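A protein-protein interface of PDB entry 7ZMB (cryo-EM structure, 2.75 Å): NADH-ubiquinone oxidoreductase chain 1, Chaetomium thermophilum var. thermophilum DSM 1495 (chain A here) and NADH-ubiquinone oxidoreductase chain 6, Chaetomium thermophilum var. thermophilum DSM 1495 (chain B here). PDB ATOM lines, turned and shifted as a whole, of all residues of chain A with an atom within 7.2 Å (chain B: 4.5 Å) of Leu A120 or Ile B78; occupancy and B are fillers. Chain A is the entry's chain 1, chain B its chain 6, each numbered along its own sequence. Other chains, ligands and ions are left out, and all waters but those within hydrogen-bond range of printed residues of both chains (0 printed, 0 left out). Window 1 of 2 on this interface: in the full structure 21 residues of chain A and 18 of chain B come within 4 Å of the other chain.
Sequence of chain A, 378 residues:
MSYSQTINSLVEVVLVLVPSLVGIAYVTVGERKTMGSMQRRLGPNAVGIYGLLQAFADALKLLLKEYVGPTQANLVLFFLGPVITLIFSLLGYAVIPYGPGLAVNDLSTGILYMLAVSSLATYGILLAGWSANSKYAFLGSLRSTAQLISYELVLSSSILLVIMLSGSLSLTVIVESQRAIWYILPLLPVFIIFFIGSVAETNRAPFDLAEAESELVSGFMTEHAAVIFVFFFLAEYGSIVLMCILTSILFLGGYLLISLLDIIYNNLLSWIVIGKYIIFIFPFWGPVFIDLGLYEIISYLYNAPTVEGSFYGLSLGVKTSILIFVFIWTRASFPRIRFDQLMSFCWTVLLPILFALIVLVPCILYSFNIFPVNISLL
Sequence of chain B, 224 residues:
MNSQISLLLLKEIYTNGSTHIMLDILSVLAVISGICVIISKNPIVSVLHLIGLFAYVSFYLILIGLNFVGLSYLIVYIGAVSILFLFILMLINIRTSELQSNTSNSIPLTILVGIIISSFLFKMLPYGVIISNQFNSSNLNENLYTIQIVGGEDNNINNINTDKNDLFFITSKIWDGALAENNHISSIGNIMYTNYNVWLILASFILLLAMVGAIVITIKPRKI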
ATOM      1  N   GLY A  81     -25.972   0.695 -29.804  1.00  0.00           N
ATOM      2  CA  GLY A  81     -24.756   0.594 -28.981  1.00  0.00           C
ATOM      3  C   GLY A  81     -23.644   1.474 -29.518  1.00  0.00           C
ATOM      4  O   GLY A  81     -23.148   2.293 -28.731  1.00  0.00           O
ATOM      5  N   ILE A  84     -24.485   5.109 -28.881  1.00  0.00           N
ATOM      6  CA  ILE A  84     -24.293   5.461 -27.475  1.00  0.00           C
ATOM      7  C   ILE A  84     -22.815   5.628 -27.157  1.00  0.00           C
ATOM      8  O   ILE A  84     -22.415   6.593 -26.497  1.00  0.00           O
ATOM      9  CB  ILE A  84     -24.956   4.424 -26.550  1.00  0.00           C
ATOM     10  CG1 ILE A  84     -26.450   4.714 -26.411  1.00  0.00           C
ATOM     11  CG2 ILE A  84     -24.262   4.363 -25.205  1.00  0.00           C
ATOM     12  CD1 ILE A  84     -27.168   3.738 -25.555  1.00  0.00           C
ATOM     13  N   THR A  85     -21.981   4.706 -27.629  1.00  0.00           N
ATOM     14  CA  THR A  85     -20.565   4.761 -27.293  1.00  0.00           C
ATOM     15  C   THR A  85     -19.914   6.019 -27.847  1.00  0.00           C
ATOM     16  O   THR A  85     -19.059   6.620 -27.192  1.00  0.00           O
ATOM     17  CB  THR A  85     -19.858   3.508 -27.806  1.00  0.00           C
ATOM     18  OG1 THR A  85     -20.614   2.359 -27.424  1.00  0.00           O
ATOM     19  CG2 THR A  85     -18.465   3.397 -27.221  1.00  0.00           C
ATOM     20  N   PHE A  88     -21.434   9.363 -25.984  1.00  0.00           N
ATOM     21  CA  PHE A  88     -21.066   9.443 -24.586  1.00  0.00           C
ATOM     22  C   PHE A  88     -19.559   9.449 -24.377  1.00  0.00           C
ATOM     23  O   PHE A  88     -19.104   9.862 -23.309  1.00  0.00           O
ATOM     24  CB  PHE A  88     -21.782   8.312 -23.854  1.00  0.00           C
ATOM     25  CG  PHE A  88     -23.191   8.665 -23.479  1.00  0.00           C
ATOM     26  CD1 PHE A  88     -23.445   9.694 -22.593  1.00  0.00           C
ATOM     27  CD2 PHE A  88     -24.260   8.095 -24.141  1.00  0.00           C
ATOM     28  CE1 PHE A  88     -24.733  10.055 -22.272  1.00  0.00           C
ATOM     29  CE2 PHE A  88     -25.563   8.463 -23.827  1.00  0.00           C
ATOM     30  CZ  PHE A  88     -25.793   9.445 -22.891  1.00  0.00           C
ATOM     31  N   SER A  89     -18.777   9.041 -25.375  1.00  0.00           N
ATOM     32  CA  SER A  89     -17.333   9.236 -25.310  1.00  0.00           C
ATOM     33  C   SER A  89     -16.950  10.686 -25.580  1.00  0.00           C
ATOM     34  O   SER A  89     -16.071  11.236 -24.909  1.00  0.00           O
ATOM     35  CB  SER A  89     -16.621   8.321 -26.308  1.00  0.00           C
ATOM     36  OG  SER A  89     -17.020   6.971 -26.157  1.00  0.00           O
ATOM     37  N   LEU A  91     -18.781  13.323 -25.115  1.00  0.00           N
ATOM     38  CA  LEU A  91     -19.307  14.246 -24.114  1.00  0.00           C
ATOM     39  C   LEU A  91     -18.251  14.615 -23.091  1.00  0.00           C
ATOM     40  O   LEU A  91     -18.318  15.692 -22.499  1.00  0.00           O
ATOM     41  CB  LEU A  91     -20.508  13.638 -23.400  1.00  0.00           C
ATOM     42  CG  LEU A  91     -21.906  13.751 -23.983  1.00  0.00           C
ATOM     43  CD1 LEU A  91     -22.882  13.257 -22.960  1.00  0.00           C
ATOM     44  CD2 LEU A  91     -22.224  15.172 -24.389  1.00  0.00           C
ATOM     45  N   MET A 114     -17.397  13.029 -15.689  1.00  0.00           N
ATOM     46  CA  MET A 114     -16.533  12.189 -16.542  1.00  0.00           C
ATOM     47  C   MET A 114     -16.683  10.707 -16.207  1.00  0.00           C
ATOM     48  O   MET A 114     -16.698   9.902 -17.142  1.00  0.00           O
ATOM     49  CB  MET A 114     -15.078  12.645 -16.425  1.00  0.00           C
ATOM     50  CG  MET A 114     -14.890  14.041 -16.968  1.00  0.00           C
ATOM     51  SD  MET A 114     -13.174  14.529 -17.148  1.00  0.00           S
ATOM     52  CE  MET A 114     -12.718  13.615 -18.620  1.00  0.00           C
ATOM     53  N   LEU A 115     -16.794  10.360 -14.930  1.00  0.00           N
ATOM     54  CA  LEU A 115     -17.036   8.946 -14.547  1.00  0.00           C
ATOM     55  C   LEU A 115     -18.391   8.471 -15.096  1.00  0.00           C
ATOM     56  O   LEU A 115     -18.439   7.365 -15.656  1.00  0.00           O
ATOM     57  CB  LEU A 115     -16.936   8.806 -13.026  1.00  0.00           C
ATOM     58  CG  LEU A 115     -15.556   9.091 -12.440  1.00  0.00           C
ATOM     59  CD1 LEU A 115     -15.586   9.074 -10.920  1.00  0.00           C
ATOM     60  CD2 LEU A 115     -14.530   8.102 -12.970  1.00  0.00           C
ATOM     61  N   ALA A 116     -19.435   9.295 -14.995  1.00  0.00           N
ATOM     62  CA  ALA A 116     -20.772   8.917 -15.499  1.00  0.00           C
ATOM     63  C   ALA A 116     -20.742   8.734 -17.017  1.00  0.00           C
ATOM     64  O   ALA A 116     -21.322   7.752 -17.503  1.00  0.00           O
ATOM     65  CB  ALA A 116     -21.790   9.941 -15.077  1.00  0.00           C
ATOM     66  N   VAL A 117     -20.090   9.645 -17.736  1.00  0.00           N
ATOM     67  CA  VAL A 117     -20.104   9.575 -19.224  1.00  0.00           C
ATOM     68  C   VAL A 117     -19.285   8.386 -19.741  1.00  0.00           C
ATOM     69  O   VAL A 117     -19.722   7.763 -20.726  1.00  0.00           O
ATOM     70  CB  VAL A 117     -19.809  10.920 -19.917  1.00  0.00           C
ATOM     71  CG1 VAL A 117     -20.878  11.959 -19.621  1.00  0.00           C
ATOM     72  CG2 VAL A 117     -18.422  11.458 -19.610  1.00  0.00           C
ATOM     73  N   SER A 118     -18.138   8.104 -19.124  1.00  0.00           N
ATOM     74  CA  SER A 118     -17.307   6.952 -19.549  1.00  0.00           C
ATOM     75  C   SER A 118     -18.038   5.632 -19.284  1.00  0.00           C
ATOM     76  O   SER A 118     -18.033   4.754 -20.168  1.00  0.00           O
ATOM     77  CB  SER A 118     -15.956   6.982 -18.901  1.00  0.00           C
ATOM     78  OG  SER A 118     -16.049   6.697 -17.513  1.00  0.00           O
ATOM     79  N   SER A 119     -18.666   5.513 -18.122  1.00  0.00           N
ATOM     80  CA  SER A 119     -19.345   4.251 -17.746  1.00  0.00           C
ATOM     81  C   SER A 119     -20.515   3.987 -18.691  1.00  0.00           C
ATOM     82  O   SER A 119     -20.786   2.812 -18.979  1.00  0.00           O
ATOM     83  CB  SER A 119     -19.778   4.271 -16.308  1.00  0.00           C
ATOM     84  OG  SER A 119     -20.695   5.326 -16.074  1.00  0.00           O
ATOM     85  N   LEU A 120     -21.169   5.042 -19.152  1.00  0.00           N
ATOM     86  CA  LEU A 120     -22.378   4.886 -19.988  1.00  0.00           C
ATOM     87  C   LEU A 120     -21.945   4.464 -21.400  1.00  0.00           C
ATOM     88  O   LEU A 120     -22.647   3.660 -22.019  1.00  0.00           O
ATOM     89  CB  LEU A 120     -23.142   6.210 -19.972  1.00  0.00           C
ATOM     90  CG  LEU A 120     -24.666   6.105 -19.948  1.00  0.00           C
ATOM     91  CD1 LEU A 120     -25.295   7.435 -19.567  1.00  0.00           C
ATOM     92  CD2 LEU A 120     -25.217   5.619 -21.280  1.00  0.00           C
ATOM     93  N   ALA A 121     -20.776   4.903 -21.836  1.00  0.00           N
ATOM     94  CA  ALA A 121     -20.327   4.580 -23.187  1.00  0.00           C
ATOM     95  C   ALA A 121     -19.837   3.143 -23.295  1.00  0.00           C
ATOM     96  O   ALA A 121     -19.947   2.534 -24.361  1.00  0.00           O
ATOM     97  CB  ALA A 121     -19.230   5.551 -23.618  1.00  0.00           C
ATOM     98  N   THR A 122     -19.288   2.590 -22.212  1.00  0.00           N
ATOM     99  CA  THR A 122     -18.895   1.187 -22.224  1.00  0.00           C
ATOM    100  C   THR A 122     -20.107   0.279 -22.319  1.00  0.00           C
ATOM    101  O   THR A 122     -20.007  -0.841 -22.829  1.00  0.00           O
ATOM    102  CB  THR A 122     -18.084   0.852 -20.976  1.00  0.00           C
ATOM    103  OG1 THR A 122     -18.887   1.067 -19.811  1.00  0.00           O
ATOM    104  CG2 THR A 122     -16.864   1.744 -20.900  1.00  0.00           C
ATOM    105  N   TYR A 123     -21.258   0.745 -21.840  1.00  0.00           N
ATOM    106  CA  TYR A 123     -22.477  -0.042 -21.958  1.00  0.00           C
ATOM    107  C   TYR A 123     -22.903  -0.201 -23.413  1.00  0.00           C
ATOM    108  O   TYR A 123     -23.543  -1.197 -23.762  1.00  0.00           O
ATOM    109  CB  TYR A 123     -23.582   0.595 -21.120  1.00  0.00           C
ATOM    110  CG  TYR A 123     -24.848  -0.206 -21.093  1.00  0.00           C
ATOM    111  CD1 TYR A 123     -24.880  -1.464 -20.518  1.00  0.00           C
ATOM    112  CD2 TYR A 123     -26.008   0.286 -21.655  1.00  0.00           C
ATOM    113  CE1 TYR A 123     -26.038  -2.210 -20.496  1.00  0.00           C
ATOM    114  CE2 TYR A 123     -27.167  -0.449 -21.642  1.00  0.00           C
ATOM    115  CZ  TYR A 123     -27.178  -1.698 -21.062  1.00  0.00           C
ATOM    116  OH  TYR A 123     -28.343  -2.429 -21.043  1.00  0.00           O
ATOM    117  N   GLY A 124     -22.555   0.754 -24.273  1.00  0.00           N
ATOM    118  CA  GLY A 124     -22.779   0.561 -25.694  1.00  0.00           C
ATOM    119  C   GLY A 124     -21.972  -0.589 -26.266  1.00  0.00           C
ATOM    120  O   GLY A 124     -22.474  -1.370 -27.073  1.00  0.00           O
ATOM    121  N   ILE A 125     -20.698  -0.680 -25.884  1.00  0.00           N
ATOM    122  CA  ILE A 125     -19.861  -1.837 -26.316  1.00  0.00           C
ATOM    123  C   ILE A 125     -20.567  -3.131 -25.893  1.00  0.00           C
ATOM    124  O   ILE A 125     -20.756  -3.998 -26.762  1.00  0.00           O
ATOM    125  CB  ILE A 125     -18.452  -1.739 -25.713  1.00  0.00           C
ATOM    126  CG1 ILE A 125     -17.671  -0.556 -26.290  1.00  0.00           C
ATOM    127  CG2 ILE A 125     -17.699  -3.049 -25.876  1.00  0.00           C
ATOM    128  CD1 ILE A 125     -16.268  -0.431 -25.753  1.00  0.00           C
ATOM    129  N   LEU A 148     -14.554  -3.694 -17.236  1.00  0.00           N
ATOM    130  CA  LEU A 148     -15.072  -2.527 -16.458  1.00  0.00           C
ATOM    131  C   LEU A 148     -15.222  -2.921 -14.986  1.00  0.00           C
ATOM    132  O   LEU A 148     -15.057  -2.045 -14.130  1.00  0.00           O
ATOM    133  CB  LEU A 148     -16.373  -1.983 -17.064  1.00  0.00           C
ATOM    134  CG  LEU A 148     -17.661  -2.765 -16.809  1.00  0.00           C
ATOM    135  CD1 LEU A 148     -18.410  -2.212 -15.605  1.00  0.00           C
ATOM    136  CD2 LEU A 148     -18.558  -2.713 -18.035  1.00  0.00           C
ATOM    137  N   GLU A 152     -12.886   0.203 -13.243  1.00  0.00           N
ATOM    138  CA  GLU A 152     -13.752   1.340 -12.811  1.00  0.00           C
ATOM    139  C   GLU A 152     -13.492   1.713 -11.353  1.00  0.00           C
ATOM    140  O   GLU A 152     -13.291   2.906 -11.074  1.00  0.00           O
ATOM    141  CB  GLU A 152     -15.227   1.014 -13.042  1.00  0.00           C
ATOM    142  CG  GLU A 152     -16.098   2.231 -13.264  1.00  0.00           C
ATOM    143  CD  GLU A 152     -17.360   2.243 -12.422  1.00  0.00           C
ATOM    144  OE1 GLU A 152     -17.353   1.610 -11.354  1.00  0.00           O
ATOM    145  OE2 GLU A 152     -18.344   2.884 -12.839  1.00  0.00           O
ATOM    146  N   ILE B  51     -31.909   1.046 -17.726  1.00  0.00           N
ATOM    147  CA  ILE B  51     -30.869   2.060 -17.611  1.00  0.00           C
ATOM    148  C   ILE B  51     -31.344   3.378 -18.203  1.00  0.00           C
ATOM    149  O   ILE B  51     -30.975   4.453 -17.718  1.00  0.00           O
ATOM    150  CB  ILE B  51     -29.543   1.573 -18.241  1.00  0.00           C
ATOM    151  CG1 ILE B  51     -28.438   2.615 -18.063  1.00  0.00           C
ATOM    152  CG2 ILE B  51     -29.701   1.232 -19.692  1.00  0.00           C
ATOM    153  CD1 ILE B  51     -28.081   2.896 -16.613  1.00  0.00           C
ATOM    154  N   LEU B  74     -26.593   7.955 -11.548  1.00  0.00           N
ATOM    155  CA  LEU B  74     -26.212   7.426 -12.883  1.00  0.00           C
ATOM    156  C   LEU B  74     -24.917   6.608 -12.754  1.00  0.00           C
ATOM    157  O   LEU B  74     -24.911   5.492 -13.249  1.00  0.00           O
ATOM    158  CB  LEU B  74     -26.053   8.626 -13.828  1.00  0.00           C
ATOM    159  CG  LEU B  74     -26.053   8.345 -15.326  1.00  0.00           C
ATOM    160  CD1 LEU B  74     -27.379   7.746 -15.763  1.00  0.00           C
ATOM    161  CD2 LEU B  74     -25.765   9.624 -16.094  1.00  0.00           C
ATOM    162  N   ILE B  75     -23.951   7.055 -11.953  1.00  0.00           N
ATOM    163  CA  ILE B  75     -22.660   6.319 -11.756  1.00  0.00           C
ATOM    164  C   ILE B  75     -22.915   4.943 -11.151  1.00  0.00           C
ATOM    165  O   ILE B  75     -22.383   3.953 -11.671  1.00  0.00           O
ATOM    166  CB  ILE B  75     -21.701   7.112 -10.844  1.00  0.00           C
ATOM    167  CG1 ILE B  75     -20.960   8.203 -11.621  1.00  0.00           C
ATOM    168  CG2 ILE B  75     -20.732   6.195 -10.116  1.00  0.00           C
ATOM    169  CD1 ILE B  75     -20.091   9.081 -10.760  1.00  0.00           C
ATOM    170  N   VAL B  76     -23.780   4.879 -10.158  1.00  0.00           N
ATOM    171  CA  VAL B  76     -23.989   3.604  -9.425  1.00  0.00           C
ATOM    172  C   VAL B  76     -24.961   2.705 -10.198  1.00  0.00           C
ATOM    173  O   VAL B  76     -24.739   1.496 -10.218  1.00  0.00           O
ATOM    174  CB  VAL B  76     -24.406   3.884  -7.966  1.00  0.00           C
ATOM    175  CG1 VAL B  76     -25.323   2.808  -7.407  1.00  0.00           C
ATOM    176  CG2 VAL B  76     -23.192   4.075  -7.078  1.00  0.00           C
ATOM    177  N   TYR B  77     -25.948   3.271 -10.870  1.00  0.00           N
ATOM    178  CA  TYR B  77     -26.947   2.388 -11.516  1.00  0.00           C
ATOM    179  C   TYR B  77     -26.507   1.972 -12.917  1.00  0.00           C
ATOM    180  O   TYR B  77     -27.148   1.074 -13.452  1.00  0.00           O
ATOM    181  CB  TYR B  77     -28.369   2.917 -11.337  1.00  0.00           C
ATOM    182  CG  TYR B  77     -28.854   2.709  -9.931  1.00  0.00           C
ATOM    183  CD1 TYR B  77     -29.198   1.449  -9.486  1.00  0.00           C
ATOM    184  CD2 TYR B  77     -28.888   3.752  -9.025  1.00  0.00           C
ATOM    185  CE1 TYR B  77     -29.598   1.236  -8.180  1.00  0.00           C
ATOM    186  CE2 TYR B  77     -29.305   3.558  -7.720  1.00  0.00           C
ATOM    187  CZ  TYR B  77     -29.666   2.294  -7.297  1.00  0.00           C
ATOM    188  OH  TYR B  77     -30.073   2.083  -6.014  1.00  0.00           O
ATOM    189  N   ILE B  78     -25.428   2.545 -13.457  1.00  0.00           N
ATOM    190  CA  ILE B  78     -24.945   2.046 -14.769  1.00  0.00           C
ATOM    191  C   ILE B  78     -24.127   0.797 -14.469  1.00  0.00           C
ATOM    192  O   ILE B  78     -24.372  -0.222 -15.132  1.00  0.00           O
ATOM    193  CB  ILE B  78     -24.134   3.113 -15.531  1.00  0.00           C
ATOM    194  CG1 ILE B  78     -24.991   4.290 -15.997  1.00  0.00           C
ATOM    195  CG2 ILE B  78     -23.378   2.501 -16.701  1.00  0.00           C
ATOM    196  CD1 ILE B  78     -24.187   5.503 -16.401  1.00  0.00           C
ATOM    197  N   GLY B  79     -23.180   0.878 -13.524  1.00  0.00           N
ATOM    198  CA  GLY B  79     -22.488  -0.327 -13.096  1.00  0.00           C
ATOM    199  C   GLY B  79     -23.435  -1.413 -12.630  1.00  0.00           C
ATOM    200  O   GLY B  79     -23.218  -2.594 -12.898  1.00  0.00           O
ATOM    201  N   ALA B  80     -24.502  -1.030 -11.930  1.00  0.00           N
ATOM    202  CA  ALA B  80     -25.472  -2.017 -11.466  1.00  0.00           C
ATOM    203  C   ALA B  80     -26.224  -2.649 -12.626  1.00  0.00           C
ATOM    204  O   ALA B  80     -26.444  -3.865 -12.638  1.00  0.00           O
ATOM    205  CB  ALA B  80     -26.449  -1.376 -10.481  1.00  0.00           C
ATOM    206  N   VAL B  81     -26.637  -1.843 -13.606  1.00  0.00           N
ATOM    207  CA  VAL B  81     -27.382  -2.384 -14.739  1.00  0.00           C
ATOM    208  C   VAL B  81     -26.491  -3.266 -15.598  1.00  0.00           C
ATOM    209  O   VAL B  81     -26.948  -4.278 -16.139  1.00  0.00           O
ATOM    210  CB  VAL B  81     -28.030  -1.244 -15.546  1.00  0.00           C
ATOM    211  CG1 VAL B  81     -28.375  -1.686 -16.945  1.00  0.00           C
ATOM    212  CG2 VAL B  81     -29.281  -0.770 -14.843  1.00  0.00           C
ATOM    213  N   SER B  82     -25.209  -2.912 -15.693  1.00  0.00           N
ATOM    214  CA  SER B  82     -24.215  -3.713 -16.447  1.00  0.00           C
ATOM    215  C   SER B  82     -24.094  -5.094 -15.796  1.00  0.00           C
ATOM    216  O   SER B  82     -24.009  -6.087 -16.525  1.00  0.00           O
ATOM    217  CB  SER B  82     -22.895  -3.021 -16.439  1.00  0.00           C
ATOM    218  OG  SER B  82     -22.982  -1.760 -17.079  1.00  0.00           O
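Of chain B, only Ile B78 comes within 4 Å of Leu A120.
Of chain A, only Ala A116 (3.8 Å), Ser A119 (3.5 Å) and Leu A120 (3.6 Å) come within 4 Å of Ile B78.
Printed residues of chain B within 4 Å of Ser A119: Ile B78.
Printed residues of chain B within 4 Å of Tyr A123: Ile B51 (3.6 Å) and Ser B82 (3.9 Å).
Of the printed residues of chain B, Leu A115 touches Ile B75 (3.9 Å).
Printed residues of chain B within 4 Å of Ala A116: Ile B75 and Ile B78.
Ala B80 touches none of the printed residues of chain A.
The nearest residue of chain B that does not touch Leu A120 is Leu B74 (4.1 Å).
O of Leu A115 sits at hydrogen-bond distance from OG of Ser A118.
O of Leu A115 is in hydrogen-bond range of OG of Ser A119, at 3.1 Å.
The side-chain hydroxyl of Ser A119 is in hydrogen-bond range of the backbone carbonyl oxygen of Ala A116, 2.9 Å away.
The side-chain hydroxyl (OG1) of Thr A122 lies within hydrogen-bond range of the backbone carbonyl oxygen (O) of Ser A119 (2.7 Å).
The side-chain hydroxyl (OG) of Ser B82 sits at hydrogen-bond distance from the backbone carbonyl oxygen (O) of Ile B78, 2.8 Å away.
Of the 10 printed residues of chain B, 4 touch a printed residue of chain A.
Along chain B the printed residues that touch a printed residue of chain A span positions 51 to 82.
Of the 20 printed residues of chain A, 5 touch a printed residue of chain B.
Among the printed residues, 7 pairs touch across the chains.
Among the printed residues, no Asp or Glu carboxylate lies within 4 Å of a Lys or Arg side-chain nitrogen of the other chain.
Among the printed residues, pairs that only touch across the chains: Leu A115 with Ile B75, Ala A116 with Ile B75, Ala A116 with Ile B78, Ser A119 with Ile B78, Leu A120 with Ile B78, Tyr A123 with Ile B51 and Tyr A123 with Ser B82.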
